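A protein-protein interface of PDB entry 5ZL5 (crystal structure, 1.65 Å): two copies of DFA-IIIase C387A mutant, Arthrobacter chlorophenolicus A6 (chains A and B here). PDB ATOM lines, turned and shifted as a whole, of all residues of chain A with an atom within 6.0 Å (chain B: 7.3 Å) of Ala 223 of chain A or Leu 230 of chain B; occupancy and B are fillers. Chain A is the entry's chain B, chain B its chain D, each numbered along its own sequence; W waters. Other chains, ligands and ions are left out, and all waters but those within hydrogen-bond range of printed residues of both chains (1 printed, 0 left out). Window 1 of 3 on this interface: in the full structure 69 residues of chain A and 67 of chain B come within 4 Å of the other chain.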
ATOM      1  N   PHE A 179       0.776   1.127  -7.471  1.00  0.00           N
ATOM      2  CA  PHE A 179       0.838   2.151  -6.431  1.00  0.00           C
ATOM      3  C   PHE A 179       0.584   3.533  -7.029  1.00  0.00           C
ATOM      4  O   PHE A 179       0.817   3.752  -8.222  1.00  0.00           O
ATOM      5  CB  PHE A 179       2.188   2.153  -5.714  1.00  0.00           C
ATOM      6  CG  PHE A 179       2.286   1.200  -4.552  1.00  0.00           C
ATOM      7  CD1 PHE A 179       1.575  -0.022  -4.517  1.00  0.00           C
ATOM      8  CD2 PHE A 179       3.134   1.502  -3.503  1.00  0.00           C
ATOM      9  CE1 PHE A 179       1.719  -0.886  -3.438  1.00  0.00           C
ATOM     10  CE2 PHE A 179       3.282   0.625  -2.424  1.00  0.00           C
ATOM     11  CZ  PHE A 179       2.570  -0.562  -2.401  1.00  0.00           C
ATOM     12  N   ALA A 198       9.135  -1.387  -8.484  1.00  0.00           N
ATOM     13  CA  ALA A 198       7.805  -0.883  -8.841  1.00  0.00           C
ATOM     14  C   ALA A 198       7.336  -1.385 -10.190  1.00  0.00           C
ATOM     15  O   ALA A 198       8.078  -1.326 -11.158  1.00  0.00           O
ATOM     16  CB  ALA A 198       7.797   0.653  -8.858  1.00  0.00           C
ATOM     17  N   ASP A 199       6.071  -1.791 -10.240  1.00  0.00           N
ATOM     18  CA  ASP A 199       5.380  -2.178 -11.475  1.00  0.00           C
ATOM     19  C   ASP A 199       4.139  -1.292 -11.583  1.00  0.00           C
ATOM     20  O   ASP A 199       3.355  -1.168 -10.642  1.00  0.00           O
ATOM     21  CB  ASP A 199       5.016  -3.658 -11.403  1.00  0.00           C
ATOM     22  CG  ASP A 199       4.394  -4.193 -12.670  1.00  0.00           C
ATOM     23  OD1 ASP A 199       4.112  -3.423 -13.624  1.00  0.00           O
ATOM     24  OD2 ASP A 199       4.172  -5.447 -12.705  1.00  0.00           O
ATOM     25  N   ALA A 200       3.981  -0.657 -12.737  1.00  0.00           N
ATOM     26  CA  ALA A 200       2.779   0.121 -13.046  1.00  0.00           C
ATOM     27  C   ALA A 200       2.432   1.150 -11.940  1.00  0.00           C
ATOM     28  O   ALA A 200       1.264   1.358 -11.560  1.00  0.00           O
ATOM     29  CB  ALA A 200       1.610  -0.817 -13.372  1.00  0.00           C
ATOM     30  N   LEU A 201       3.491   1.808 -11.479  1.00  0.00           N
ATOM     31  CA  LEU A 201       3.424   2.877 -10.505  1.00  0.00           C
ATOM     32  C   LEU A 201       3.089   4.202 -11.203  1.00  0.00           C
ATOM     33  O   LEU A 201       3.587   4.447 -12.297  1.00  0.00           O
ATOM     34  CB  LEU A 201       4.809   2.997  -9.840  1.00  0.00           C
ATOM     35  CG  LEU A 201       5.119   4.277  -9.074  1.00  0.00           C
ATOM     36  CD1 LEU A 201       4.345   4.382  -7.764  1.00  0.00           C
ATOM     37  CD2 LEU A 201       6.622   4.332  -8.848  1.00  0.00           C
ATOM     38  N   SER A 202       2.289   5.043 -10.545  1.00  0.00           N
ATOM     39  CA  SER A 202       2.051   6.440 -10.998  1.00  0.00           C
ATOM     40  C   SER A 202       2.390   7.451  -9.897  1.00  0.00           C
ATOM     41  O   SER A 202       1.797   7.415  -8.805  1.00  0.00           O
ATOM     42  CB  SER A 202       0.626   6.651 -11.429  1.00  0.00           C
ATOM     43  OG  SER A 202       0.511   7.950 -12.013  1.00  0.00           O
ATOM     44  N   GLY A 221      12.182  -2.053 -12.181  1.00  0.00           N
ATOM     45  CA  GLY A 221      10.775  -1.750 -12.324  1.00  0.00           C
ATOM     46  C   GLY A 221      10.312  -1.798 -13.757  1.00  0.00           C
ATOM     47  O   GLY A 221      11.103  -1.981 -14.690  1.00  0.00           O
ATOM     48  N   GLN A 222       9.012  -1.692 -13.921  1.00  0.00           N
ATOM     49  CA  GLN A 222       8.426  -1.697 -15.255  1.00  0.00           C
ATOM     50  C   GLN A 222       7.143  -0.894 -15.333  1.00  0.00           C
ATOM     51  O   GLN A 222       6.447  -0.725 -14.342  1.00  0.00           O
ATOM     52  CB  GLN A 222       8.178  -3.136 -15.760  1.00  0.00           C
ATOM     53  CG  GLN A 222       7.167  -3.937 -14.994  1.00  0.00           C
ATOM     54  CD  GLN A 222       6.887  -5.279 -15.684  1.00  0.00           C
ATOM     55  OE1 GLN A 222       7.431  -5.569 -16.764  1.00  0.00           O
ATOM     56  NE2 GLN A 222       6.048  -6.085 -15.077  1.00  0.00           N
ATOM     57  N   ALA A 223       6.859  -0.437 -16.545  1.00  0.00           N
ATOM     58  CA  ALA A 223       5.568   0.121 -16.943  1.00  0.00           C
ATOM     59  C   ALA A 223       5.061   1.217 -16.005  1.00  0.00           C
ATOM     60  O   ALA A 223       3.856   1.331 -15.766  1.00  0.00           O
ATOM     61  CB  ALA A 223       4.517  -0.986 -17.133  1.00  0.00           C
ATOM     62  N   SER A 224       5.987   2.046 -15.517  1.00  0.00           N
ATOM     63  CA  SER A 224       5.624   3.103 -14.574  1.00  0.00           C
ATOM     64  C   SER A 224       5.612   4.490 -15.217  1.00  0.00           C
ATOM     65  O   SER A 224       6.026   4.667 -16.381  1.00  0.00           O
ATOM     66  CB  SER A 224       6.567   3.042 -13.384  1.00  0.00           C
ATOM     67  OG  SER A 224       6.427   1.793 -12.682  1.00  0.00           O
ATOM     68  N   LYS A 225       5.106   5.474 -14.476  1.00  0.00           N
ATOM     69  CA  LYS A 225       5.067   6.835 -14.985  1.00  0.00           C
ATOM     70  C   LYS A 225       5.223   7.882 -13.896  1.00  0.00           C
ATOM     71  O   LYS A 225       4.783   7.712 -12.747  1.00  0.00           O
ATOM     72  CB  LYS A 225       3.846   7.107 -15.852  1.00  0.00           C
ATOM     73  CG  LYS A 225       2.535   6.969 -15.172  1.00  0.00           C
ATOM     74  CD  LYS A 225       1.420   7.206 -16.193  1.00  0.00           C
ATOM     75  CE  LYS A 225       0.056   6.900 -15.620  1.00  0.00           C
ATOM     76  NZ  LYS A 225      -0.428   7.960 -14.705  1.00  0.00           N
ATOM     77  N   HIS A 245      14.823   0.049 -14.844  1.00  0.00           N
ATOM     78  CA  HIS A 245      13.439   0.179 -15.251  1.00  0.00           C
ATOM     79  C   HIS A 245      13.320  -0.015 -16.753  1.00  0.00           C
ATOM     80  O   HIS A 245      14.179   0.433 -17.509  1.00  0.00           O
ATOM     81  CB  HIS A 245      12.870   1.545 -14.885  1.00  0.00           C
ATOM     82  CG  HIS A 245      12.158   1.562 -13.574  1.00  0.00           C
ATOM     83  ND1 HIS A 245      10.793   1.702 -13.479  1.00  0.00           N
ATOM     84  CD2 HIS A 245      12.616   1.425 -12.307  1.00  0.00           C
ATOM     85  CE1 HIS A 245      10.440   1.685 -12.212  1.00  0.00           C
ATOM     86  NE2 HIS A 245      11.526   1.508 -11.477  1.00  0.00           N
ATOM     87  N   GLY A 246      12.251  -0.702 -17.172  1.00  0.00           N
ATOM     88  CA  GLY A 246      11.861  -0.740 -18.558  1.00  0.00           C
ATOM     89  C   GLY A 246      10.489  -0.098 -18.724  1.00  0.00           C
ATOM     90  O   GLY A 246       9.622  -0.238 -17.865  1.00  0.00           O
ATOM     91  N   GLY A 247      10.282   0.603 -19.827  1.00  0.00           N
ATOM     92  CA  GLY A 247       8.965   1.166 -20.103  1.00  0.00           C
ATOM     93  C   GLY A 247       8.494   2.254 -19.158  1.00  0.00           C
ATOM     94  O   GLY A 247       7.312   2.362 -18.895  1.00  0.00           O
ATOM     95  N   LEU A 248       9.429   3.026 -18.627  1.00  0.00           N
ATOM     96  CA  LEU A 248       9.118   4.167 -17.789  1.00  0.00           C
ATOM     97  C   LEU A 248       8.770   5.363 -18.676  1.00  0.00           C
ATOM     98  O   LEU A 248       9.448   5.611 -19.676  1.00  0.00           O
ATOM     99  CB  LEU A 248      10.332   4.515 -16.928  1.00  0.00           C
ATOM    100  CG  LEU A 248      10.214   5.697 -15.957  1.00  0.00           C
ATOM    101  CD1 LEU A 248       9.135   5.477 -14.927  1.00  0.00           C
ATOM    102  CD2 LEU A 248      11.580   5.926 -15.324  1.00  0.00           C
ATOM    103  N   MET B 184      -9.826   5.903 -11.508  1.00  0.00           N
ATOM    104  CA  MET B 184     -10.519   4.603 -11.385  1.00  0.00           C
ATOM    105  C   MET B 184      -9.564   3.423 -11.475  1.00  0.00           C
ATOM    106  O   MET B 184      -8.434   3.553 -11.962  1.00  0.00           O
ATOM    107  CB  MET B 184     -11.569   4.469 -12.477  1.00  0.00           C
ATOM    108  CG  MET B 184     -12.677   5.530 -12.403  1.00  0.00           C
ATOM    109  SD  MET B 184     -13.813   5.331 -11.022  1.00  0.00           S
ATOM    110  CE  MET B 184     -14.518   3.741 -11.439  1.00  0.00           C
ATOM    111  N   HIS B 205      -5.875   9.731 -15.661  1.00  0.00           N
ATOM    112  CA  HIS B 205      -5.225   9.095 -14.526  1.00  0.00           C
ATOM    113  C   HIS B 205      -5.971   7.896 -13.956  1.00  0.00           C
ATOM    114  O   HIS B 205      -6.134   7.776 -12.759  1.00  0.00           O
ATOM    115  CB  HIS B 205      -4.888  10.130 -13.442  1.00  0.00           C
ATOM    116  CG  HIS B 205      -3.786   9.683 -12.535  1.00  0.00           C
ATOM    117  ND1 HIS B 205      -4.018   9.236 -11.258  1.00  0.00           N
ATOM    118  CD2 HIS B 205      -2.454   9.578 -12.736  1.00  0.00           C
ATOM    119  CE1 HIS B 205      -2.864   8.911 -10.695  1.00  0.00           C
ATOM    120  NE2 HIS B 205      -1.904   9.107 -11.570  1.00  0.00           N
ATOM    121  N   ASN B 206      -6.428   7.013 -14.838  1.00  0.00           N
ATOM    122  CA  ASN B 206      -7.034   5.765 -14.428  1.00  0.00           C
ATOM    123  C   ASN B 206      -6.053   4.610 -14.546  1.00  0.00           C
ATOM    124  O   ASN B 206      -5.011   4.727 -15.185  1.00  0.00           O
ATOM    125  CB  ASN B 206      -8.279   5.470 -15.264  1.00  0.00           C
ATOM    126  CG  ASN B 206      -9.290   6.599 -15.206  1.00  0.00           C
ATOM    127  OD1 ASN B 206     -10.040   6.717 -14.237  1.00  0.00           O
ATOM    128  ND2 ASN B 206      -9.304   7.450 -16.241  1.00  0.00           N
ATOM    129  N   PHE B 207      -6.443   3.481 -13.960  1.00  0.00           N
ATOM    130  CA  PHE B 207      -5.741   2.219 -14.104  1.00  0.00           C
ATOM    131  C   PHE B 207      -6.753   1.219 -14.656  1.00  0.00           C
ATOM    132  O   PHE B 207      -7.698   0.812 -13.946  1.00  0.00           O
ATOM    133  CB  PHE B 207      -5.193   1.785 -12.755  1.00  0.00           C
ATOM    134  CG  PHE B 207      -4.151   0.719 -12.846  1.00  0.00           C
ATOM    135  CD1 PHE B 207      -4.507  -0.625 -13.034  1.00  0.00           C
ATOM    136  CD2 PHE B 207      -2.809   1.045 -12.741  1.00  0.00           C
ATOM    137  CE1 PHE B 207      -3.530  -1.613 -13.121  1.00  0.00           C
ATOM    138  CE2 PHE B 207      -1.842   0.062 -12.830  1.00  0.00           C
ATOM    139  CZ  PHE B 207      -2.206  -1.269 -13.032  1.00  0.00           C
ATOM    140  N   ILE B 208      -6.578   0.879 -15.931  1.00  0.00           N
ATOM    141  CA  ILE B 208      -7.561   0.099 -16.688  1.00  0.00           C
ATOM    142  C   ILE B 208      -6.843  -1.097 -17.270  1.00  0.00           C
ATOM    143  O   ILE B 208      -6.212  -0.995 -18.302  1.00  0.00           O
ATOM    144  CB  ILE B 208      -8.225   0.960 -17.789  1.00  0.00           C
ATOM    145  CG1 ILE B 208      -8.440   2.397 -17.285  1.00  0.00           C
ATOM    146  CG2 ILE B 208      -9.510   0.287 -18.258  1.00  0.00           C
ATOM    147  CD1 ILE B 208      -9.092   3.285 -18.324  1.00  0.00           C
ATOM    148  N   ALA B 209      -6.926  -2.243 -16.594  1.00  0.00           N
ATOM    149  CA  ALA B 209      -6.050  -3.373 -16.930  1.00  0.00           C
ATOM    150  C   ALA B 209      -6.766  -4.711 -16.770  1.00  0.00           C
ATOM    151  O   ALA B 209      -7.686  -4.834 -15.956  1.00  0.00           O
ATOM    152  CB  ALA B 209      -4.801  -3.347 -16.061  1.00  0.00           C
ATOM    153  N   CYS B 214     -10.391  -1.830 -23.054  1.00  0.00           N
ATOM    154  CA  CYS B 214     -10.290  -0.841 -22.005  1.00  0.00           C
ATOM    155  C   CYS B 214     -11.145   0.387 -22.297  1.00  0.00           C
ATOM    156  O   CYS B 214     -12.269   0.467 -21.821  1.00  0.00           O
ATOM    157  CB  CYS B 214      -8.822  -0.540 -21.747  1.00  0.00           C
ATOM    158  SG  CYS B 214      -8.004  -2.007 -21.090  1.00  0.00           S
ATOM    159  N   ILE B 215     -10.647   1.304 -23.112  1.00  0.00           N
ATOM    160  CA  ILE B 215     -11.364   2.549 -23.408  1.00  0.00           C
ATOM    161  C   ILE B 215     -11.876   2.527 -24.862  1.00  0.00           C
ATOM    162  O   ILE B 215     -11.076   2.400 -25.800  1.00  0.00           O
ATOM    163  CB  ILE B 215     -10.442   3.775 -23.271  1.00  0.00           C
ATOM    164  CG1 ILE B 215      -9.881   3.885 -21.849  1.00  0.00           C
ATOM    165  CG2 ILE B 215     -11.182   5.041 -23.719  1.00  0.00           C
ATOM    166  CD1 ILE B 215      -8.695   4.833 -21.732  1.00  0.00           C
ATOM    167  N   THR B 227      -5.732  10.977 -21.068  1.00  0.00           N
ATOM    168  CA  THR B 227      -4.417  11.368 -20.562  1.00  0.00           C
ATOM    169  C   THR B 227      -4.000  10.664 -19.283  1.00  0.00           C
ATOM    170  O   THR B 227      -4.802  10.446 -18.382  1.00  0.00           O
ATOM    171  CB  THR B 227      -4.328  12.900 -20.317  1.00  0.00           C
ATOM    172  OG1 THR B 227      -5.206  13.280 -19.259  1.00  0.00           O
ATOM    173  CG2 THR B 227      -4.680  13.679 -21.565  1.00  0.00           C
ATOM    174  N   ASP B 228      -2.719  10.310 -19.218  1.00  0.00           N
ATOM    175  CA  ASP B 228      -2.080   9.861 -17.968  1.00  0.00           C
ATOM    176  C   ASP B 228      -2.667   8.567 -17.431  1.00  0.00           C
ATOM    177  O   ASP B 228      -2.711   8.356 -16.222  1.00  0.00           O
ATOM    178  CB  ASP B 228      -2.176  10.988 -16.923  1.00  0.00           C
ATOM    179  CG  ASP B 228      -0.821  11.363 -16.344  1.00  0.00           C
ATOM    180  OD1 ASP B 228      -0.169  10.524 -15.671  1.00  0.00           O
ATOM    181  OD2 ASP B 228      -0.412  12.515 -16.577  1.00  0.00           O
ATOM    182  N   ASN B 229      -3.134   7.708 -18.333  1.00  0.00           N
ATOM    183  CA  ASN B 229      -3.736   6.422 -17.934  1.00  0.00           C
ATOM    184  C   ASN B 229      -2.704   5.293 -18.055  1.00  0.00           C
ATOM    185  O   ASN B 229      -1.784   5.339 -18.867  1.00  0.00           O
ATOM    186  CB  ASN B 229      -4.955   6.082 -18.805  1.00  0.00           C
ATOM    187  CG  ASN B 229      -6.045   7.104 -18.686  1.00  0.00           C
ATOM    188  OD1 ASN B 229      -6.767   7.148 -17.684  1.00  0.00           O
ATOM    189  ND2 ASN B 229      -6.188   7.929 -19.702  1.00  0.00           N
ATOM    190  N   LEU B 230      -2.875   4.291 -17.214  1.00  0.00           N
ATOM    191  CA  LEU B 230      -2.179   3.018 -17.330  1.00  0.00           C
ATOM    192  C   LEU B 230      -3.213   2.026 -17.871  1.00  0.00           C
ATOM    193  O   LEU B 230      -4.279   1.885 -17.282  1.00  0.00           O
ATOM    194  CB  LEU B 230      -1.683   2.591 -15.948  1.00  0.00           C
ATOM    195  CG  LEU B 230      -0.339   3.215 -15.591  1.00  0.00           C
ATOM    196  CD1 LEU B 230      -0.139   3.412 -14.100  1.00  0.00           C
ATOM    197  CD2 LEU B 230       0.792   2.362 -16.172  1.00  0.00           C
ATOM    198  N   VAL B 231      -2.906   1.397 -19.004  1.00  0.00           N
ATOM    199  CA  VAL B 231      -3.884   0.655 -19.790  1.00  0.00           C
ATOM    200  C   VAL B 231      -3.321  -0.669 -20.292  1.00  0.00           C
ATOM    201  O   VAL B 231      -2.256  -0.682 -20.897  1.00  0.00           O
ATOM    202  CB  VAL B 231      -4.335   1.453 -21.027  1.00  0.00           C
ATOM    203  CG1 VAL B 231      -5.484   0.744 -21.740  1.00  0.00           C
ATOM    204  CG2 VAL B 231      -4.770   2.852 -20.646  1.00  0.00           C
ATOM    205  N   GLY B 232      -4.063  -1.760 -20.081  1.00  0.00           N
ATOM    206  CA  GLY B 232      -3.677  -3.088 -20.620  1.00  0.00           C
ATOM    207  C   GLY B 232      -4.930  -3.908 -20.934  1.00  0.00           C
ATOM    208  O   GLY B 232      -5.749  -4.166 -20.054  1.00  0.00           O
ATOM    209  N   ALA B 252       0.400  11.019 -22.852  1.00  0.00           N
ATOM    210  CA  ALA B 252       0.955  10.670 -21.525  1.00  0.00           C
ATOM    211  C   ALA B 252       0.361   9.384 -20.932  1.00  0.00           C
ATOM    212  O   ALA B 252       0.308   9.223 -19.719  1.00  0.00           O
ATOM    213  CB  ALA B 252       0.817  11.847 -20.571  1.00  0.00           C
ATOM    214  N   ASN B 253      -0.087   8.476 -21.800  1.00  0.00           N
ATOM    215  CA  ASN B 253      -0.542   7.164 -21.392  1.00  0.00           C
ATOM    216  C   ASN B 253       0.611   6.165 -21.469  1.00  0.00           C
ATOM    217  O   ASN B 253       1.500   6.285 -22.316  1.00  0.00           O
ATOM    218  CB  ASN B 253      -1.712   6.704 -22.247  1.00  0.00           C
ATOM    219  CG  ASN B 253      -2.861   7.690 -22.224  1.00  0.00           C
ATOM    220  OD1 ASN B 253      -3.597   7.768 -21.237  1.00  0.00           O
ATOM    221  ND2 ASN B 253      -3.034   8.430 -23.308  1.00  0.00           N
ATOM    222  N   ASN B 254       0.581   5.221 -20.544  1.00  0.00           N
ATOM    223  CA  ASN B 254       1.452   4.056 -20.548  1.00  0.00           C
ATOM    224  C   ASN B 254       0.582   2.852 -20.827  1.00  0.00           C
ATOM    225  O   ASN B 254      -0.171   2.383 -19.953  1.00  0.00           O
ATOM    226  CB  ASN B 254       2.199   3.944 -19.226  1.00  0.00           C
ATOM    227  CG  ASN B 254       3.357   2.993 -19.296  1.00  0.00           C
ATOM    228  OD1 ASN B 254       3.245   1.911 -19.865  1.00  0.00           O
ATOM    229  ND2 ASN B 254       4.500   3.401 -18.747  1.00  0.00           N
ATOM    230  N   VAL B 255       0.632   2.418 -22.083  1.00  0.00           N
ATOM    231  CA  VAL B 255      -0.189   1.319 -22.583  1.00  0.00           C
ATOM    232  C   VAL B 255       0.708   0.094 -22.670  1.00  0.00           C
ATOM    233  O   VAL B 255       1.699   0.090 -23.408  1.00  0.00           O
ATOM    234  CB  VAL B 255      -0.803   1.633 -23.957  1.00  0.00           C
ATOM    235  CG1 VAL B 255      -1.751   0.520 -24.386  1.00  0.00           C
ATOM    236  CG2 VAL B 255      -1.575   2.942 -23.921  1.00  0.00           C
ATOM    237  N   PHE B 256       0.357  -0.940 -21.918  1.00  0.00           N
ATOM    238  CA  PHE B 256       1.152  -2.177 -21.879  1.00  0.00           C
ATOM    239  C   PHE B 256       0.288  -3.301 -22.422  1.00  0.00           C
ATOM    240  O   PHE B 256      -0.868  -3.083 -22.750  1.00  0.00           O
ATOM    241  CB  PHE B 256       1.690  -2.434 -20.468  1.00  0.00           C
ATOM    242  CG  PHE B 256       0.673  -2.247 -19.373  1.00  0.00           C
ATOM    243  CD1 PHE B 256      -0.258  -3.239 -19.081  1.00  0.00           C
ATOM    244  CD2 PHE B 256       0.637  -1.066 -18.642  1.00  0.00           C
ATOM    245  CE1 PHE B 256      -1.186  -3.074 -18.066  1.00  0.00           C
ATOM    246  CE2 PHE B 256      -0.294  -0.903 -17.626  1.00  0.00           C
ATOM    247  CZ  PHE B 256      -1.203  -1.904 -17.339  1.00  0.00           C
ATOM    248  N   PRO B 257       0.858  -4.506 -22.601  1.00  0.00           N
ATOM    249  CA  PRO B 257       0.062  -5.556 -23.259  1.00  0.00           C
ATOM    250  C   PRO B 257      -1.197  -5.968 -22.477  1.00  0.00           C
ATOM    251  O   PRO B 257      -1.293  -5.681 -21.282  1.00  0.00           O
ATOM    252  CB  PRO B 257       1.069  -6.697 -23.410  1.00  0.00           C
ATOM    253  CG  PRO B 257       2.384  -5.992 -23.506  1.00  0.00           C
ATOM    254  CD  PRO B 257       2.283  -4.852 -22.555  1.00  0.00           C
ATOM    255  N   ARG B 277       3.738   6.024 -24.116  1.00  0.00           N
ATOM    256  CA  ARG B 277       4.582   4.836 -24.131  1.00  0.00           C
ATOM    257  C   ARG B 277       3.655   3.675 -24.441  1.00  0.00           C
ATOM    258  O   ARG B 277       2.659   3.462 -23.738  1.00  0.00           O
ATOM    259  CB  ARG B 277       5.284   4.665 -22.799  1.00  0.00           C
ATOM    260  CG  ARG B 277       6.216   3.449 -22.730  1.00  0.00           C
ATOM    261  CD  ARG B 277       5.489   2.236 -22.187  1.00  0.00           C
ATOM    262  NE  ARG B 277       6.306   1.031 -22.243  1.00  0.00           N
ATOM    263  CZ  ARG B 277       6.077  -0.091 -21.558  1.00  0.00           C
ATOM    264  NH1 ARG B 277       5.058  -0.198 -20.716  1.00  0.00           N
ATOM    265  NH2 ARG B 277       6.920  -1.127 -21.712  1.00  0.00           N
ATOM    266  N   HIS B 279       3.483  -0.448 -25.483  1.00  0.00           N
ATOM    267  CA  HIS B 279       4.158  -1.749 -25.529  1.00  0.00           C
ATOM    268  C   HIS B 279       3.153  -2.827 -25.949  1.00  0.00           C
ATOM    269  O   HIS B 279       2.101  -2.966 -25.326  1.00  0.00           O
ATOM    270  CB  HIS B 279       4.747  -2.063 -24.169  1.00  0.00           C
ATOM    271  CG  HIS B 279       5.370  -3.422 -24.076  1.00  0.00           C
ATOM    272  ND1 HIS B 279       5.534  -4.065 -22.873  1.00  0.00           N
ATOM    273  CD2 HIS B 279       5.855  -4.259 -25.021  1.00  0.00           C
ATOM    274  CE1 HIS B 279       6.100  -5.241 -23.074  1.00  0.00           C
ATOM    275  NE2 HIS B 279       6.308  -5.380 -24.365  1.00  0.00           N
ATOM    276  N   VAL B 392       9.734  -8.113 -16.532  1.00  0.00           N
ATOM    277  CA  VAL B 392      10.841  -7.180 -16.232  1.00  0.00           C
ATOM    278  C   VAL B 392      12.131  -7.620 -16.927  1.00  0.00           C
ATOM    279  O   VAL B 392      12.816  -6.801 -17.559  1.00  0.00           O
ATOM    280  CB  VAL B 392      11.086  -6.975 -14.702  1.00  0.00           C
ATOM    281  CG1 VAL B 392      12.284  -6.056 -14.444  1.00  0.00           C
ATOM    282  CG2 VAL B 392       9.861  -6.366 -14.031  1.00  0.00           C
ATOM    283  N   LEU B 395      12.029  -6.896 -20.657  1.00  0.00           N
ATOM    284  CA  LEU B 395      12.187  -5.466 -20.954  1.00  0.00           C
ATOM    285  C   LEU B 395      13.643  -4.992 -20.872  1.00  0.00           C
ATOM    286  O   LEU B 395      14.079  -4.138 -21.671  1.00  0.00           O
ATOM    287  CB  LEU B 395      11.329  -4.625 -20.008  1.00  0.00           C
ATOM    288  CG  LEU B 395       9.847  -4.532 -20.340  1.00  0.00           C
ATOM    289  CD1 LEU B 395       9.128  -3.756 -19.249  1.00  0.00           C
ATOM    290  CD2 LEU B 395       9.620  -3.863 -21.685  1.00  0.00           C
HETATM  291  O   HOH W   1      -2.924   6.248 -13.688  1.00  0.00           O
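OG of Ser 202 of chain A sits at hydrogen-bond distance from NE2 of His 205 of chain B (2.7 Å).
OE1 of Gln 222 of chain A lies within hydrogen-bond range of N of Val 392 of chain B (3.4 Å).
O of Gly 247 of chain A lies within hydrogen-bond range of ND2 of Asn 254 of chain B (3.0 Å).
The side-chain amide nitrogen of Asn 254 of chain B lies within hydrogen-bond range of the backbone carbonyl oxygen of Ser 224 of chain A (3.1 Å).
The side-chain carboxylate of Asp 228 of chain B is in salt-bridge range of the side-chain amino group of Lys 225 of chain A, at 2.8 Å.
The backbone NH (N) of His 205 of chain B lies close to the backbone carbonyl oxygen (O) of Asp 228 of chain B (3.5 Å).
N of Ala 200 of chain A sits at hydrogen-bond distance from OG of Ser 224 of chain A (3.5 Å).
The backbone NH (N) of Leu 201 of chain A sits at hydrogen-bond distance from the side-chain hydroxyl (OG) of Ser 224 of chain A, 3.2 Å away.
N of Ala 200 of chain A sits at hydrogen-bond distance from O of Gln 222 of chain A, 2.9 Å away.
The backbone carbonyl oxygen (O) of Gly 221 of chain A lies within hydrogen-bond range of the backbone NH (N) of Gly 246 of chain A, 3.0 Å away.
N of His 205 of chain B sits at hydrogen-bond distance from OD1 of Asn 229 of chain B (3.4 Å).
Among the printed residues, pairs that only touch across the chains: Lys 225 of chain A with His 205 of chain B, Ala 223 of chain A with Leu 230 of chain B, Gly 247 of chain A with Arg 277 of chain B, Gln 222 of chain A with Leu 395 of chain B, Ala 223 of chain A with Asn 254 of chain B, Ala 200 of chain A with Leu 230 of chain B, Ala 200 of chain A with Phe 207 of chain B, Lys 225 of chain A with Leu 230 of chain B, Ala 223 of chain A with Arg 277 of chain B and Gly 246 of chain A with Leu 395 of chain B.
Printed residues of chain B within 4 Å of Ser 202 of chain A: His 205.
Of chain B, only Leu 230 (3.3 Å), Asn 254 (3.6 Å) and Arg 277 (3.7 Å) come within 4 Å of Ala 223 of chain A.
Printed residues of chain B within 4 Å of Ser 224 of chain A: Asn 254.
Of the printed residues of chain A, His 205 of chain B touches Ser 202 and Lys 225.
Ile 208 of chain B touches none of the printed residues of chain A.
Of the printed residues of chain A, Leu 230 of chain B touches Ala 200, Ala 223 and Lys 225.
Printed residues of chain A within 4 Å of Asn 254 of chain B: Ala 223 (3.6 Å), Ser 224 (3.1 Å) and Gly 247 (3.0 Å).
Of the printed residues of chain A, Val 392 of chain B touches Gln 222 (3.4 Å).
The nearest residue of chain B that does not touch Ala 223 of chain A is Phe 256 of chain B (4.2 Å).
Of the 15 printed residues of chain A, 8 touch a printed residue of chain B.
Printed residues of chain A that touch a printed residue of chain B: Ala 200, Ser 202, Gln 222, Ala 223, Ser 224, Lys 225, Gly 246 and Gly 247.
Along chain B the printed residues that touch a printed residue of chain A span positions 205 to 395.
Among the printed residues, 15 pairs touch across the chains.
No position is printed for both chains.
Of the 15 pairs that touch across the chains among the printed residues, none has its exchanged pair printed and touching as well.
Water W1 lies within hydrogen-bond range of the backbone carbonyl oxygen (O) of Asn 206 of chain B, the side-chain amino group (NZ) of Lys 225 of chain A and the backbone carbonyl oxygen (O) of Asp 228 of chain B.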
